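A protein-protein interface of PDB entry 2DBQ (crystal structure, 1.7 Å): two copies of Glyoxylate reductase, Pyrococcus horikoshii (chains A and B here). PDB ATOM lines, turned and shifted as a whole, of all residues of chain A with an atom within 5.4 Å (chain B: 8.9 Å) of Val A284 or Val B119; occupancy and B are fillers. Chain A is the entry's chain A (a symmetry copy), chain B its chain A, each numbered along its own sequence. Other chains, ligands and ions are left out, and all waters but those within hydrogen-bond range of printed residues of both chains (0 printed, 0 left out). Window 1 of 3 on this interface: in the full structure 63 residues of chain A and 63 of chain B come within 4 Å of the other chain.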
ATOM      1  N   LEU A 107      15.334 -24.736  -8.679  1.00  0.00           N
ATOM      2  CA  LEU A 107      16.376 -25.630  -8.185  1.00  0.00           C
ATOM      3  C   LEU A 107      16.296 -26.991  -8.873  1.00  0.00           C
ATOM      4  O   LEU A 107      17.321 -27.607  -9.151  1.00  0.00           O
ATOM      5  CB  LEU A 107      16.281 -25.829  -6.668  1.00  0.00           C
ATOM      6  CG  LEU A 107      17.450 -26.713  -6.204  1.00  0.00           C
ATOM      7  CD1 LEU A 107      18.703 -25.861  -6.090  1.00  0.00           C
ATOM      8  CD2 LEU A 107      17.134 -27.387  -4.884  1.00  0.00           C
ATOM      9  N   ALA A 110      18.032 -26.634 -11.936  1.00  0.00           N
ATOM     10  CA  ALA A 110      19.449 -26.396 -11.670  1.00  0.00           C
ATOM     11  C   ALA A 110      20.136 -27.755 -11.503  1.00  0.00           C
ATOM     12  O   ALA A 110      21.225 -27.979 -12.027  1.00  0.00           O
ATOM     13  CB  ALA A 110      19.621 -25.562 -10.408  1.00  0.00           C
ATOM     14  N   LEU A 111      19.493 -28.665 -10.779  1.00  0.00           N
ATOM     15  CA  LEU A 111      20.065 -29.996 -10.570  1.00  0.00           C
ATOM     16  C   LEU A 111      20.054 -30.829 -11.854  1.00  0.00           C
ATOM     17  O   LEU A 111      21.001 -31.562 -12.135  1.00  0.00           O
ATOM     18  CB  LEU A 111      19.297 -30.745  -9.472  1.00  0.00           C
ATOM     19  CG  LEU A 111      19.448 -30.223  -8.038  1.00  0.00           C
ATOM     20  CD1 LEU A 111      18.500 -30.987  -7.118  1.00  0.00           C
ATOM     21  CD2 LEU A 111      20.899 -30.366  -7.584  1.00  0.00           C
ATOM     22  N   ALA A 114      22.878 -29.355 -13.997  1.00  0.00           N
ATOM     23  CA  ALA A 114      24.180 -29.588 -13.384  1.00  0.00           C
ATOM     24  C   ALA A 114      24.583 -31.060 -13.478  1.00  0.00           C
ATOM     25  O   ALA A 114      25.747 -31.379 -13.720  1.00  0.00           O
ATOM     26  CB  ALA A 114      24.159 -29.136 -11.922  1.00  0.00           C
ATOM     27  N   THR A 115      23.615 -31.952 -13.293  1.00  0.00           N
ATOM     28  CA  THR A 115      23.879 -33.384 -13.348  1.00  0.00           C
ATOM     29  C   THR A 115      24.138 -33.818 -14.785  1.00  0.00           C
ATOM     30  O   THR A 115      25.079 -34.565 -15.062  1.00  0.00           O
ATOM     31  CB  THR A 115      22.687 -34.194 -12.785  1.00  0.00           C
ATOM     32  OG1 THR A 115      22.373 -33.725 -11.469  1.00  0.00           O
ATOM     33  CG2 THR A 115      23.036 -35.680 -12.709  1.00  0.00           C
ATOM     34  N   VAL A 120      29.430 -29.678 -11.428  1.00  0.00           N
ATOM     35  CA  VAL A 120      30.150 -29.795 -10.156  1.00  0.00           C
ATOM     36  C   VAL A 120      31.538 -30.400 -10.362  1.00  0.00           C
ATOM     37  O   VAL A 120      32.530 -29.934  -9.791  1.00  0.00           O
ATOM     38  CB  VAL A 120      29.373 -30.660  -9.141  1.00  0.00           C
ATOM     39  CG1 VAL A 120      30.180 -30.800  -7.855  1.00  0.00           C
ATOM     40  CG2 VAL A 120      28.025 -30.013  -8.836  1.00  0.00           C
ATOM     41  N   ALA A 262      22.250 -38.772 -11.069  1.00  0.00           N
ATOM     42  CA  ALA A 262      21.142 -38.324 -10.241  1.00  0.00           C
ATOM     43  C   ALA A 262      21.452 -37.022  -9.539  1.00  0.00           C
ATOM     44  O   ALA A 262      22.591 -36.783  -9.128  1.00  0.00           O
ATOM     45  CB  ALA A 262      20.794 -39.398  -9.214  1.00  0.00           C
ATOM     46  N   GLY A 263      20.430 -36.179  -9.423  1.00  0.00           N
ATOM     47  CA  GLY A 263      20.559 -34.903  -8.740  1.00  0.00           C
ATOM     48  C   GLY A 263      19.586 -34.978  -7.578  1.00  0.00           C
ATOM     49  O   GLY A 263      18.375 -35.113  -7.786  1.00  0.00           O
ATOM     50  N   LEU A 264      20.102 -34.883  -6.355  1.00  0.00           N
ATOM     51  CA  LEU A 264      19.267 -35.006  -5.162  1.00  0.00           C
ATOM     52  C   LEU A 264      19.337 -33.829  -4.187  1.00  0.00           C
ATOM     53  O   LEU A 264      20.425 -33.419  -3.773  1.00  0.00           O
ATOM     54  CB  LEU A 264      19.651 -36.295  -4.424  1.00  0.00           C
ATOM     55  CG  LEU A 264      19.835 -37.527  -5.327  1.00  0.00           C
ATOM     56  CD1 LEU A 264      20.540 -38.643  -4.554  1.00  0.00           C
ATOM     57  CD2 LEU A 264      18.480 -37.991  -5.861  1.00  0.00           C
ATOM     58  N   ASN A 282      28.900 -38.909 -10.657  1.00  0.00           N
ATOM     59  CA  ASN A 282      27.765 -38.657 -11.542  1.00  0.00           C
ATOM     60  C   ASN A 282      26.499 -38.279 -10.764  1.00  0.00           C
ATOM     61  O   ASN A 282      25.378 -38.444 -11.248  1.00  0.00           O
ATOM     62  CB  ASN A 282      27.510 -39.862 -12.464  1.00  0.00           C
ATOM     63  CG  ASN A 282      27.181 -41.132 -11.708  1.00  0.00           C
ATOM     64  OD1 ASN A 282      27.630 -41.332 -10.581  1.00  0.00           O
ATOM     65  ND2 ASN A 282      26.410 -42.009 -12.339  1.00  0.00           N
ATOM     66  N   VAL A 283      26.691 -37.776  -9.548  1.00  0.00           N
ATOM     67  CA  VAL A 283      25.576 -37.321  -8.728  1.00  0.00           C
ATOM     68  C   VAL A 283      25.864 -35.893  -8.279  1.00  0.00           C
ATOM     69  O   VAL A 283      27.022 -35.493  -8.143  1.00  0.00           O
ATOM     70  CB  VAL A 283      25.356 -38.202  -7.453  1.00  0.00           C
ATOM     71  CG1 VAL A 283      25.199 -39.657  -7.847  1.00  0.00           C
ATOM     72  CG2 VAL A 283      26.507 -38.020  -6.464  1.00  0.00           C
ATOM     73  N   VAL A 284      24.804 -35.121  -8.074  1.00  0.00           N
ATOM     74  CA  VAL A 284      24.917 -33.750  -7.599  1.00  0.00           C
ATOM     75  C   VAL A 284      24.018 -33.719  -6.369  1.00  0.00           C
ATOM     76  O   VAL A 284      22.880 -34.179  -6.425  1.00  0.00           O
ATOM     77  CB  VAL A 284      24.419 -32.735  -8.644  1.00  0.00           C
ATOM     78  CG1 VAL A 284      24.472 -31.337  -8.068  1.00  0.00           C
ATOM     79  CG2 VAL A 284      25.279 -32.816  -9.899  1.00  0.00           C
ATOM     80  N   LEU A 285      24.532 -33.185  -5.264  1.00  0.00           N
ATOM     81  CA  LEU A 285      23.794 -33.146  -4.003  1.00  0.00           C
ATOM     82  C   LEU A 285      23.668 -31.746  -3.423  1.00  0.00           C
ATOM     83  O   LEU A 285      24.605 -30.956  -3.480  1.00  0.00           O
ATOM     84  CB  LEU A 285      24.515 -34.011  -2.973  1.00  0.00           C
ATOM     85  CG  LEU A 285      25.063 -35.347  -3.467  1.00  0.00           C
ATOM     86  CD1 LEU A 285      26.204 -35.793  -2.550  1.00  0.00           C
ATOM     87  CD2 LEU A 285      23.943 -36.378  -3.516  1.00  0.00           C
ATOM     88  N   THR A 286      22.503 -31.445  -2.859  1.00  0.00           N
ATOM     89  CA  THR A 286      22.275 -30.160  -2.211  1.00  0.00           C
ATOM     90  C   THR A 286      21.497 -30.464  -0.927  1.00  0.00           C
ATOM     91  O   THR A 286      20.682 -31.384  -0.887  1.00  0.00           O
ATOM     92  CB  THR A 286      21.505 -29.161  -3.132  1.00  0.00           C
ATOM     93  OG1 THR A 286      20.298 -29.762  -3.615  1.00  0.00           O
ATOM     94  CG2 THR A 286      22.379 -28.764  -4.319  1.00  0.00           C
ATOM     95  N   ILE A 289      17.744 -27.376  -0.177  1.00  0.00           N
ATOM     96  CA  ILE A 289      17.730 -25.940  -0.415  1.00  0.00           C
ATOM     97  C   ILE A 289      16.727 -25.565  -1.507  1.00  0.00           C
ATOM     98  O   ILE A 289      16.827 -24.500  -2.110  1.00  0.00           O
ATOM     99  CB  ILE A 289      19.134 -25.427  -0.832  1.00  0.00           C
ATOM    100  CG1 ILE A 289      19.580 -26.096  -2.137  1.00  0.00           C
ATOM    101  CG2 ILE A 289      20.131 -25.699   0.275  1.00  0.00           C
ATOM    102  CD1 ILE A 289      20.916 -25.600  -2.662  1.00  0.00           C
ATOM    103  N   PHE B 109      22.476 -21.817 -19.131  1.00  0.00           N
ATOM    104  CA  PHE B 109      21.459 -21.817 -18.090  1.00  0.00           C
ATOM    105  C   PHE B 109      21.870 -22.659 -16.893  1.00  0.00           C
ATOM    106  O   PHE B 109      21.460 -22.377 -15.767  1.00  0.00           O
ATOM    107  CB  PHE B 109      20.100 -22.286 -18.625  1.00  0.00           C
ATOM    108  CG  PHE B 109      19.068 -21.196 -18.634  1.00  0.00           C
ATOM    109  CD1 PHE B 109      19.034 -20.263 -19.670  1.00  0.00           C
ATOM    110  CD2 PHE B 109      18.200 -21.035 -17.558  1.00  0.00           C
ATOM    111  CE1 PHE B 109      18.153 -19.179 -19.629  1.00  0.00           C
ATOM    112  CE2 PHE B 109      17.317 -19.955 -17.505  1.00  0.00           C
ATOM    113  CZ  PHE B 109      17.295 -19.025 -18.541  1.00  0.00           C
ATOM    114  N   ALA B 110      22.676 -23.694 -17.133  1.00  0.00           N
ATOM    115  CA  ALA B 110      23.160 -24.540 -16.044  1.00  0.00           C
ATOM    116  C   ALA B 110      24.014 -23.674 -15.113  1.00  0.00           C
ATOM    117  O   ALA B 110      23.902 -23.763 -13.892  1.00  0.00           O
ATOM    118  CB  ALA B 110      23.988 -25.693 -16.594  1.00  0.00           C
ATOM    119  N   LEU B 111      24.860 -22.829 -15.692  1.00  0.00           N
ATOM    120  CA  LEU B 111      25.713 -21.954 -14.886  1.00  0.00           C
ATOM    121  C   LEU B 111      24.905 -20.859 -14.186  1.00  0.00           C
ATOM    122  O   LEU B 111      25.176 -20.516 -13.036  1.00  0.00           O
ATOM    123  CB  LEU B 111      26.796 -21.306 -15.759  1.00  0.00           C
ATOM    124  CG  LEU B 111      27.894 -22.227 -16.303  1.00  0.00           C
ATOM    125  CD1 LEU B 111      28.784 -21.444 -17.265  1.00  0.00           C
ATOM    126  CD2 LEU B 111      28.705 -22.807 -15.146  1.00  0.00           C
ATOM    127  N   LEU B 112      23.916 -20.313 -14.884  1.00  0.00           N
ATOM    128  CA  LEU B 112      23.078 -19.257 -14.326  1.00  0.00           C
ATOM    129  C   LEU B 112      22.373 -19.774 -13.070  1.00  0.00           C
ATOM    130  O   LEU B 112      22.387 -19.127 -12.018  1.00  0.00           O
ATOM    131  CB  LEU B 112      22.052 -18.804 -15.374  1.00  0.00           C
ATOM    132  CG  LEU B 112      21.165 -17.592 -15.061  1.00  0.00           C
ATOM    133  CD1 LEU B 112      20.585 -17.053 -16.363  1.00  0.00           C
ATOM    134  CD2 LEU B 112      20.051 -17.975 -14.088  1.00  0.00           C
ATOM    135  N   LEU B 113      21.776 -20.954 -13.184  1.00  0.00           N
ATOM    136  CA  LEU B 113      21.065 -21.561 -12.063  1.00  0.00           C
ATOM    137  C   LEU B 113      22.000 -22.020 -10.945  1.00  0.00           C
ATOM    138  O   LEU B 113      21.726 -21.795  -9.767  1.00  0.00           O
ATOM    139  CB  LEU B 113      20.221 -22.737 -12.564  1.00  0.00           C
ATOM    140  CG  LEU B 113      19.018 -22.321 -13.419  1.00  0.00           C
ATOM    141  CD1 LEU B 113      18.426 -23.526 -14.117  1.00  0.00           C
ATOM    142  CD2 LEU B 113      17.982 -21.645 -12.535  1.00  0.00           C
ATOM    143  N   ALA B 114      23.106 -22.660 -11.312  1.00  0.00           N
ATOM    144  CA  ALA B 114      24.056 -23.147 -10.320  1.00  0.00           C
ATOM    145  C   ALA B 114      24.655 -21.997  -9.512  1.00  0.00           C
ATOM    146  O   ALA B 114      24.850 -22.112  -8.302  1.00  0.00           O
ATOM    147  CB  ALA B 114      25.166 -23.948 -11.006  1.00  0.00           C
ATOM    148  N   THR B 115      24.939 -20.886 -10.184  1.00  0.00           N
ATOM    149  CA  THR B 115      25.523 -19.725  -9.525  1.00  0.00           C
ATOM    150  C   THR B 115      24.487 -19.042  -8.642  1.00  0.00           C
ATOM    151  O   THR B 115      24.766 -18.685  -7.496  1.00  0.00           O
ATOM    152  CB  THR B 115      26.055 -18.703 -10.559  1.00  0.00           C
ATOM    153  OG1 THR B 115      26.958 -19.361 -11.455  1.00  0.00           O
ATOM    154  CG2 THR B 115      26.797 -17.567  -9.858  1.00  0.00           C
ATOM    155  N   ALA B 116      23.284 -18.869  -9.174  1.00  0.00           N
ATOM    156  CA  ALA B 116      22.222 -18.218  -8.422  1.00  0.00           C
ATOM    157  C   ALA B 116      21.824 -18.984  -7.160  1.00  0.00           C
ATOM    158  O   ALA B 116      21.508 -18.378  -6.136  1.00  0.00           O
ATOM    159  CB  ALA B 116      20.991 -18.032  -9.313  1.00  0.00           C
ATOM    160  N   ARG B 117      21.862 -20.312  -7.227  1.00  0.00           N
ATOM    161  CA  ARG B 117      21.419 -21.128  -6.103  1.00  0.00           C
ATOM    162  C   ARG B 117      22.473 -21.870  -5.288  1.00  0.00           C
ATOM    163  O   ARG B 117      22.137 -22.718  -4.464  1.00  0.00           O
ATOM    164  CB  ARG B 117      20.338 -22.097  -6.595  1.00  0.00           C
ATOM    165  CG  ARG B 117      19.115 -21.369  -7.180  1.00  0.00           C
ATOM    166  CD  ARG B 117      18.433 -20.499  -6.125  1.00  0.00           C
ATOM    167  NE  ARG B 117      17.879 -21.337  -5.072  1.00  0.00           N
ATOM    168  CZ  ARG B 117      16.692 -21.930  -5.134  1.00  0.00           C
ATOM    169  NH1 ARG B 117      15.914 -21.760  -6.196  1.00  0.00           N
ATOM    170  NH2 ARG B 117      16.301 -22.731  -4.150  1.00  0.00           N
ATOM    171  N   HIS B 118      23.740 -21.544  -5.514  1.00  0.00           N
ATOM    172  CA  HIS B 118      24.841 -22.140  -4.762  1.00  0.00           C
ATOM    173  C   HIS B 118      24.906 -23.661  -4.814  1.00  0.00           C
ATOM    174  O   HIS B 118      25.226 -24.300  -3.812  1.00  0.00           O
ATOM    175  CB  HIS B 118      24.749 -21.703  -3.295  1.00  0.00           C
ATOM    176  CG  HIS B 118      24.632 -20.222  -3.112  1.00  0.00           C
ATOM    177  ND1 HIS B 118      25.666 -19.353  -3.392  1.00  0.00           N
ATOM    178  CD2 HIS B 118      23.596 -19.454  -2.698  1.00  0.00           C
ATOM    179  CE1 HIS B 118      25.272 -18.113  -3.159  1.00  0.00           C
ATOM    180  NE2 HIS B 118      24.018 -18.147  -2.738  1.00  0.00           N
ATOM    181  N   VAL B 119      24.629 -24.242  -5.977  1.00  0.00           N
ATOM    182  CA  VAL B 119      24.652 -25.695  -6.111  1.00  0.00           C
ATOM    183  C   VAL B 119      26.029 -26.321  -5.852  1.00  0.00           C
ATOM    184  O   VAL B 119      26.122 -27.355  -5.187  1.00  0.00           O
ATOM    185  CB  VAL B 119      24.144 -26.122  -7.510  1.00  0.00           C
ATOM    186  CG1 VAL B 119      24.259 -27.636  -7.678  1.00  0.00           C
ATOM    187  CG2 VAL B 119      22.696 -25.687  -7.684  1.00  0.00           C
ATOM    188  N   VAL B 120      27.094 -25.709  -6.369  1.00  0.00           N
ATOM    189  CA  VAL B 120      28.441 -26.253  -6.169  1.00  0.00           C
ATOM    190  C   VAL B 120      28.836 -26.217  -4.693  1.00  0.00           C
ATOM    191  O   VAL B 120      29.396 -27.180  -4.157  1.00  0.00           O
ATOM    192  CB  VAL B 120      29.496 -25.477  -6.987  1.00  0.00           C
ATOM    193  CG1 VAL B 120      30.885 -26.038  -6.707  1.00  0.00           C
ATOM    194  CG2 VAL B 120      29.182 -25.592  -8.475  1.00  0.00           C
ATOM    195  N   LYS B 121      28.534 -25.100  -4.043  1.00  0.00           N
ATOM    196  CA  LYS B 121      28.826 -24.911  -2.627  1.00  0.00           C
ATOM    197  C   LYS B 121      28.009 -25.913  -1.806  1.00  0.00           C
ATOM    198  O   LYS B 121      28.521 -26.534  -0.874  1.00  0.00           O
ATOM    199  CB  LYS B 121      28.468 -23.475  -2.232  1.00  0.00           C
ATOM    200  CG  LYS B 121      28.859 -23.058  -0.830  1.00  0.00           C
ATOM    201  CD  LYS B 121      28.383 -21.633  -0.560  1.00  0.00           C
ATOM    202  CE  LYS B 121      28.676 -21.204   0.869  1.00  0.00           C
ATOM    203  NZ  LYS B 121      28.080 -19.865   1.146  1.00  0.00           N
ATOM    204  N   GLY B 122      26.737 -26.072  -2.165  1.00  0.00           N
ATOM    205  CA  GLY B 122      25.879 -27.002  -1.453  1.00  0.00           C
ATOM    206  C   GLY B 122      26.350 -28.439  -1.598  1.00  0.00           C
ATOM    207  O   GLY B 122      26.332 -29.210  -0.634  1.00  0.00           O
ATOM    208  N   ASP B 123      26.774 -28.807  -2.805  1.00  0.00           N
ATOM    209  CA  ASP B 123      27.252 -30.160  -3.056  1.00  0.00           C
ATOM    210  C   ASP B 123      28.486 -30.477  -2.207  1.00  0.00           C
ATOM    211  O   ASP B 123      28.602 -31.566  -1.640  1.00  0.00           O
ATOM    212  CB  ASP B 123      27.573 -30.336  -4.543  1.00  0.00           C
ATOM    213  CG  ASP B 123      28.061 -31.732  -4.870  1.00  0.00           C
ATOM    214  OD1 ASP B 123      29.236 -32.030  -4.574  1.00  0.00           O
ATOM    215  OD2 ASP B 123      27.272 -32.539  -5.407  1.00  0.00           O
ATOM    216  N   ARG B 124      29.399 -29.517  -2.119  1.00  0.00           N
ATOM    217  CA  ARG B 124      30.617 -29.679  -1.337  1.00  0.00           C
ATOM    218  C   ARG B 124      30.282 -29.877   0.141  1.00  0.00           C
ATOM    219  O   ARG B 124      30.868 -30.723   0.822  1.00  0.00           O
ATOM    220  CB  ARG B 124      31.492 -28.439  -1.506  1.00  0.00           C
ATOM    221  CG  ARG B 124      32.728 -28.408  -0.635  1.00  0.00           C
ATOM    222  CD  ARG B 124      33.778 -29.386  -1.102  1.00  0.00           C
ATOM    223  NE  ARG B 124      35.096 -28.755  -1.114  1.00  0.00           N
ATOM    224  CZ  ARG B 124      36.237 -29.397  -1.352  1.00  0.00           C
ATOM    225  NH1 ARG B 124      36.225 -30.702  -1.599  1.00  0.00           N
ATOM    226  NH2 ARG B 124      37.389 -28.734  -1.352  1.00  0.00           N
ATOM    227  N   PHE B 125      29.328 -29.087   0.622  1.00  0.00           N
ATOM    228  CA  PHE B 125      28.879 -29.134   2.013  1.00  0.00           C
ATOM    229  C   PHE B 125      28.327 -30.513   2.388  1.00  0.00           C
ATOM    230  O   PHE B 125      28.602 -31.039   3.470  1.00  0.00           O
ATOM    231  CB  PHE B 125      27.806 -28.062   2.225  1.00  0.00           C
ATOM    232  CG  PHE B 125      27.275 -27.990   3.626  1.00  0.00           C
ATOM    233  CD1 PHE B 125      28.118 -27.672   4.691  1.00  0.00           C
ATOM    234  CD2 PHE B 125      25.923 -28.201   3.878  1.00  0.00           C
ATOM    235  CE1 PHE B 125      27.618 -27.562   5.989  1.00  0.00           C
ATOM    236  CE2 PHE B 125      25.410 -28.094   5.170  1.00  0.00           C
ATOM    237  CZ  PHE B 125      26.257 -27.773   6.230  1.00  0.00           C
ATOM    238  N   VAL B 126      27.540 -31.092   1.490  1.00  0.00           N
ATOM    239  CA  VAL B 126      26.959 -32.406   1.723  1.00  0.00           C
ATOM    240  C   VAL B 126      28.002 -33.502   1.534  1.00  0.00           C
ATOM    241  O   VAL B 126      28.281 -34.277   2.450  1.00  0.00           O
ATOM    242  CB  VAL B 126      25.792 -32.685   0.746  1.00  0.00           C
ATOM    243  CG1 VAL B 126      25.251 -34.091   0.973  1.00  0.00           C
ATOM    244  CG2 VAL B 126      24.700 -31.640   0.926  1.00  0.00           C
ATOM    245  N   ARG B 127      28.578 -33.539   0.336  1.00  0.00           N
ATOM    246  CA  ARG B 127      29.564 -34.539  -0.057  1.00  0.00           C
ATOM    247  C   ARG B 127      30.785 -34.680   0.849  1.00  0.00           C
ATOM    248  O   ARG B 127      31.299 -35.786   1.024  1.00  0.00           O
ATOM    249  CB  ARG B 127      30.029 -34.257  -1.486  1.00  0.00           C
ATOM    250  CG  ARG B 127      30.805 -35.394  -2.136  1.00  0.00           C
ATOM    251  CD  ARG B 127      31.310 -34.973  -3.512  1.00  0.00           C
ATOM    252  NE  ARG B 127      30.223 -34.622  -4.425  1.00  0.00           N
ATOM    253  CZ  ARG B 127      29.550 -35.502  -5.157  1.00  0.00           C
ATOM    254  NH1 ARG B 127      29.851 -36.791  -5.088  1.00  0.00           N
ATOM    255  NH2 ARG B 127      28.581 -35.090  -5.963  1.00  0.00           N
ATOM    256  N   PHE B 143      22.637 -21.256   2.147  1.00  0.00           N
ATOM    257  CA  PHE B 143      22.611 -21.291   0.684  1.00  0.00           C
ATOM    258  C   PHE B 143      21.495 -20.454   0.066  1.00  0.00           C
ATOM    259  O   PHE B 143      20.985 -20.763  -1.014  1.00  0.00           O
ATOM    260  CB  PHE B 143      22.508 -22.751   0.232  1.00  0.00           C
ATOM    261  CG  PHE B 143      23.539 -23.640   0.866  1.00  0.00           C
ATOM    262  CD1 PHE B 143      24.874 -23.564   0.478  1.00  0.00           C
ATOM    263  CD2 PHE B 143      23.190 -24.505   1.906  1.00  0.00           C
ATOM    264  CE1 PHE B 143      25.851 -24.329   1.114  1.00  0.00           C
ATOM    265  CE2 PHE B 143      24.158 -25.274   2.551  1.00  0.00           C
ATOM    266  CZ  PHE B 143      25.491 -25.186   2.154  1.00  0.00           C
ATOM    267  N   GLY B 145      19.728 -18.152  -2.081  1.00  0.00           N
ATOM    268  CA  GLY B 145      20.083 -17.674  -3.400  1.00  0.00           C
ATOM    269  C   GLY B 145      19.051 -16.805  -4.088  1.00  0.00           C
ATOM    270  O   GLY B 145      18.026 -16.433  -3.515  1.00  0.00           O
ATOM    271  N   ASP B 281      33.588 -18.282  -3.172  1.00  0.00           N
ATOM    272  CA  ASP B 281      32.548 -19.298  -3.177  1.00  0.00           C
ATOM    273  C   ASP B 281      31.291 -18.853  -3.921  1.00  0.00           C
ATOM    274  O   ASP B 281      30.306 -19.589  -3.955  1.00  0.00           O
ATOM    275  CB  ASP B 281      32.181 -19.711  -1.750  1.00  0.00           C
ATOM    276  CG  ASP B 281      31.785 -18.535  -0.884  1.00  0.00           C
ATOM    277  OD1 ASP B 281      31.487 -17.451  -1.435  1.00  0.00           O
ATOM    278  OD2 ASP B 281      31.763 -18.702   0.355  1.00  0.00           O
ATOM    279  N   VAL B 283      31.313 -18.084  -7.196  1.00  0.00           N
ATOM    280  CA  VAL B 283      31.588 -18.270  -8.614  1.00  0.00           C
ATOM    281  C   VAL B 283      31.488 -19.759  -8.929  1.00  0.00           C
ATOM    282  O   VAL B 283      31.730 -20.606  -8.068  1.00  0.00           O
ATOM    283  CB  VAL B 283      33.013 -17.774  -9.030  1.00  0.00           C
ATOM    284  CG1 VAL B 283      33.205 -16.331  -8.612  1.00  0.00           C
ATOM    285  CG2 VAL B 283      34.095 -18.670  -8.427  1.00  0.00           C
ATOM    286  N   VAL B 284      31.106 -20.069 -10.161  1.00  0.00           N
ATOM    287  CA  VAL B 284      31.009 -21.445 -10.625  1.00  0.00           C
ATOM    288  C   VAL B 284      31.868 -21.464 -11.884  1.00  0.00           C
ATOM    289  O   VAL B 284      31.725 -20.594 -12.740  1.00  0.00           O
ATOM    290  CB  VAL B 284      29.560 -21.838 -10.967  1.00  0.00           C
ATOM    291  CG1 VAL B 284      29.528 -23.242 -11.529  1.00  0.00           C
ATOM    292  CG2 VAL B 284      28.690 -21.753  -9.720  1.00  0.00           C
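NH1 of Arg B117 touches N of Leu A107, at 3.9 Å. Ala A110 touches Leu B113 (CB to CB, 3.6 Å). Asp B123 touches Val A120 (OD1 to CG1, 3.6 Å). Val B119 touches Val A284 (CG1 to CG1, 3.7 Å). CA of Val A284 touches OD2 of Asp B123 (3.4 Å). Leu A285 touches Gly B122. Thr A286 touches Val B126. CD2 of Phe B143 touches CG2 of Ile A289 (3.7 Å).
Of the printed residues of chain B, Ala A110 touches Leu B113. No residue of chain B comes within 4 Å of Gly A263. Of the printed residues of chain B, Val A283 touches Arg B127. Val A284 touches just these residues of chain B: Val B119 (3.7 Å) and Asp B123 (3.4 Å). Of the printed residues of chain B, Leu A285 touches Gly B122 and Asp B123. Of the printed residues of chain A, Arg B117 touches Leu A107 (3.9 Å) and Ile A289 (2.8 Å). Of the printed residues of chain A, Val B119 touches Val A284. Printed residues of chain A within 4 Å of Asp B123: Val A120 (3.6 Å), Val A284 (3.4 Å) and Leu A285 (2.8 Å). Printed residues of chain A within 4 Å of Val B126: Thr A286 (3.9 Å). Asp B281 touches none of the printed residues of chain A. The nearest residue of chain B that does not touch Val A284 is Arg B127 (4.2 Å). The nearest printed residue of chain A that does not touch Val B119 is Thr A286 (4.01 Å).
Positions printed for both chains: 110, 111, 114, 115, 120, 283 and 284. Of the 11 pairs that touch across the chains among the printed residues, none has its exchanged pair printed and touching as well.
Of the 24 printed residues of chain B, 8 touch a printed residue of chain A. Hydrophobic or aromatic side chains of chain B that line the printed part of chain A: Leu B113, Val B119, Val B126 and Phe B143. Among the printed residues, no Asp or Glu carboxylate lies within 4 Å of a Lys or Arg side-chain nitrogen of the other chain.
The backbone NH (N) of Val B119 sits at hydrogen-bond distance from the backbone carbonyl oxygen (O) of Ala B114. OD1 of Asp B123 is in salt-bridge range of NE of Arg B127. The backbone carbonyl oxygen of Ala A262 lies within hydrogen-bond range of the backbone NH of Val A284, 3.0 Å away. O of Val A284 is in hydrogen-bond range of N of Leu A264, 2.9 Å away. O of Leu A264 sits at hydrogen-bond distance from N of Thr A286 (3.0 Å).
The guanidinium group (NH2) of Arg B117 is in hydrogen-bond range of the backbone carbonyl oxygen (O) of Ile A289 (2.8 Å). OD2 of Asp B123 lies within hydrogen-bond range of N of Leu A285 (2.8 Å). The guanidinium group (NH2) of Arg B127 sits at hydrogen-bond distance from the backbone carbonyl oxygen (O) of Val A283, at 2.7 Å.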
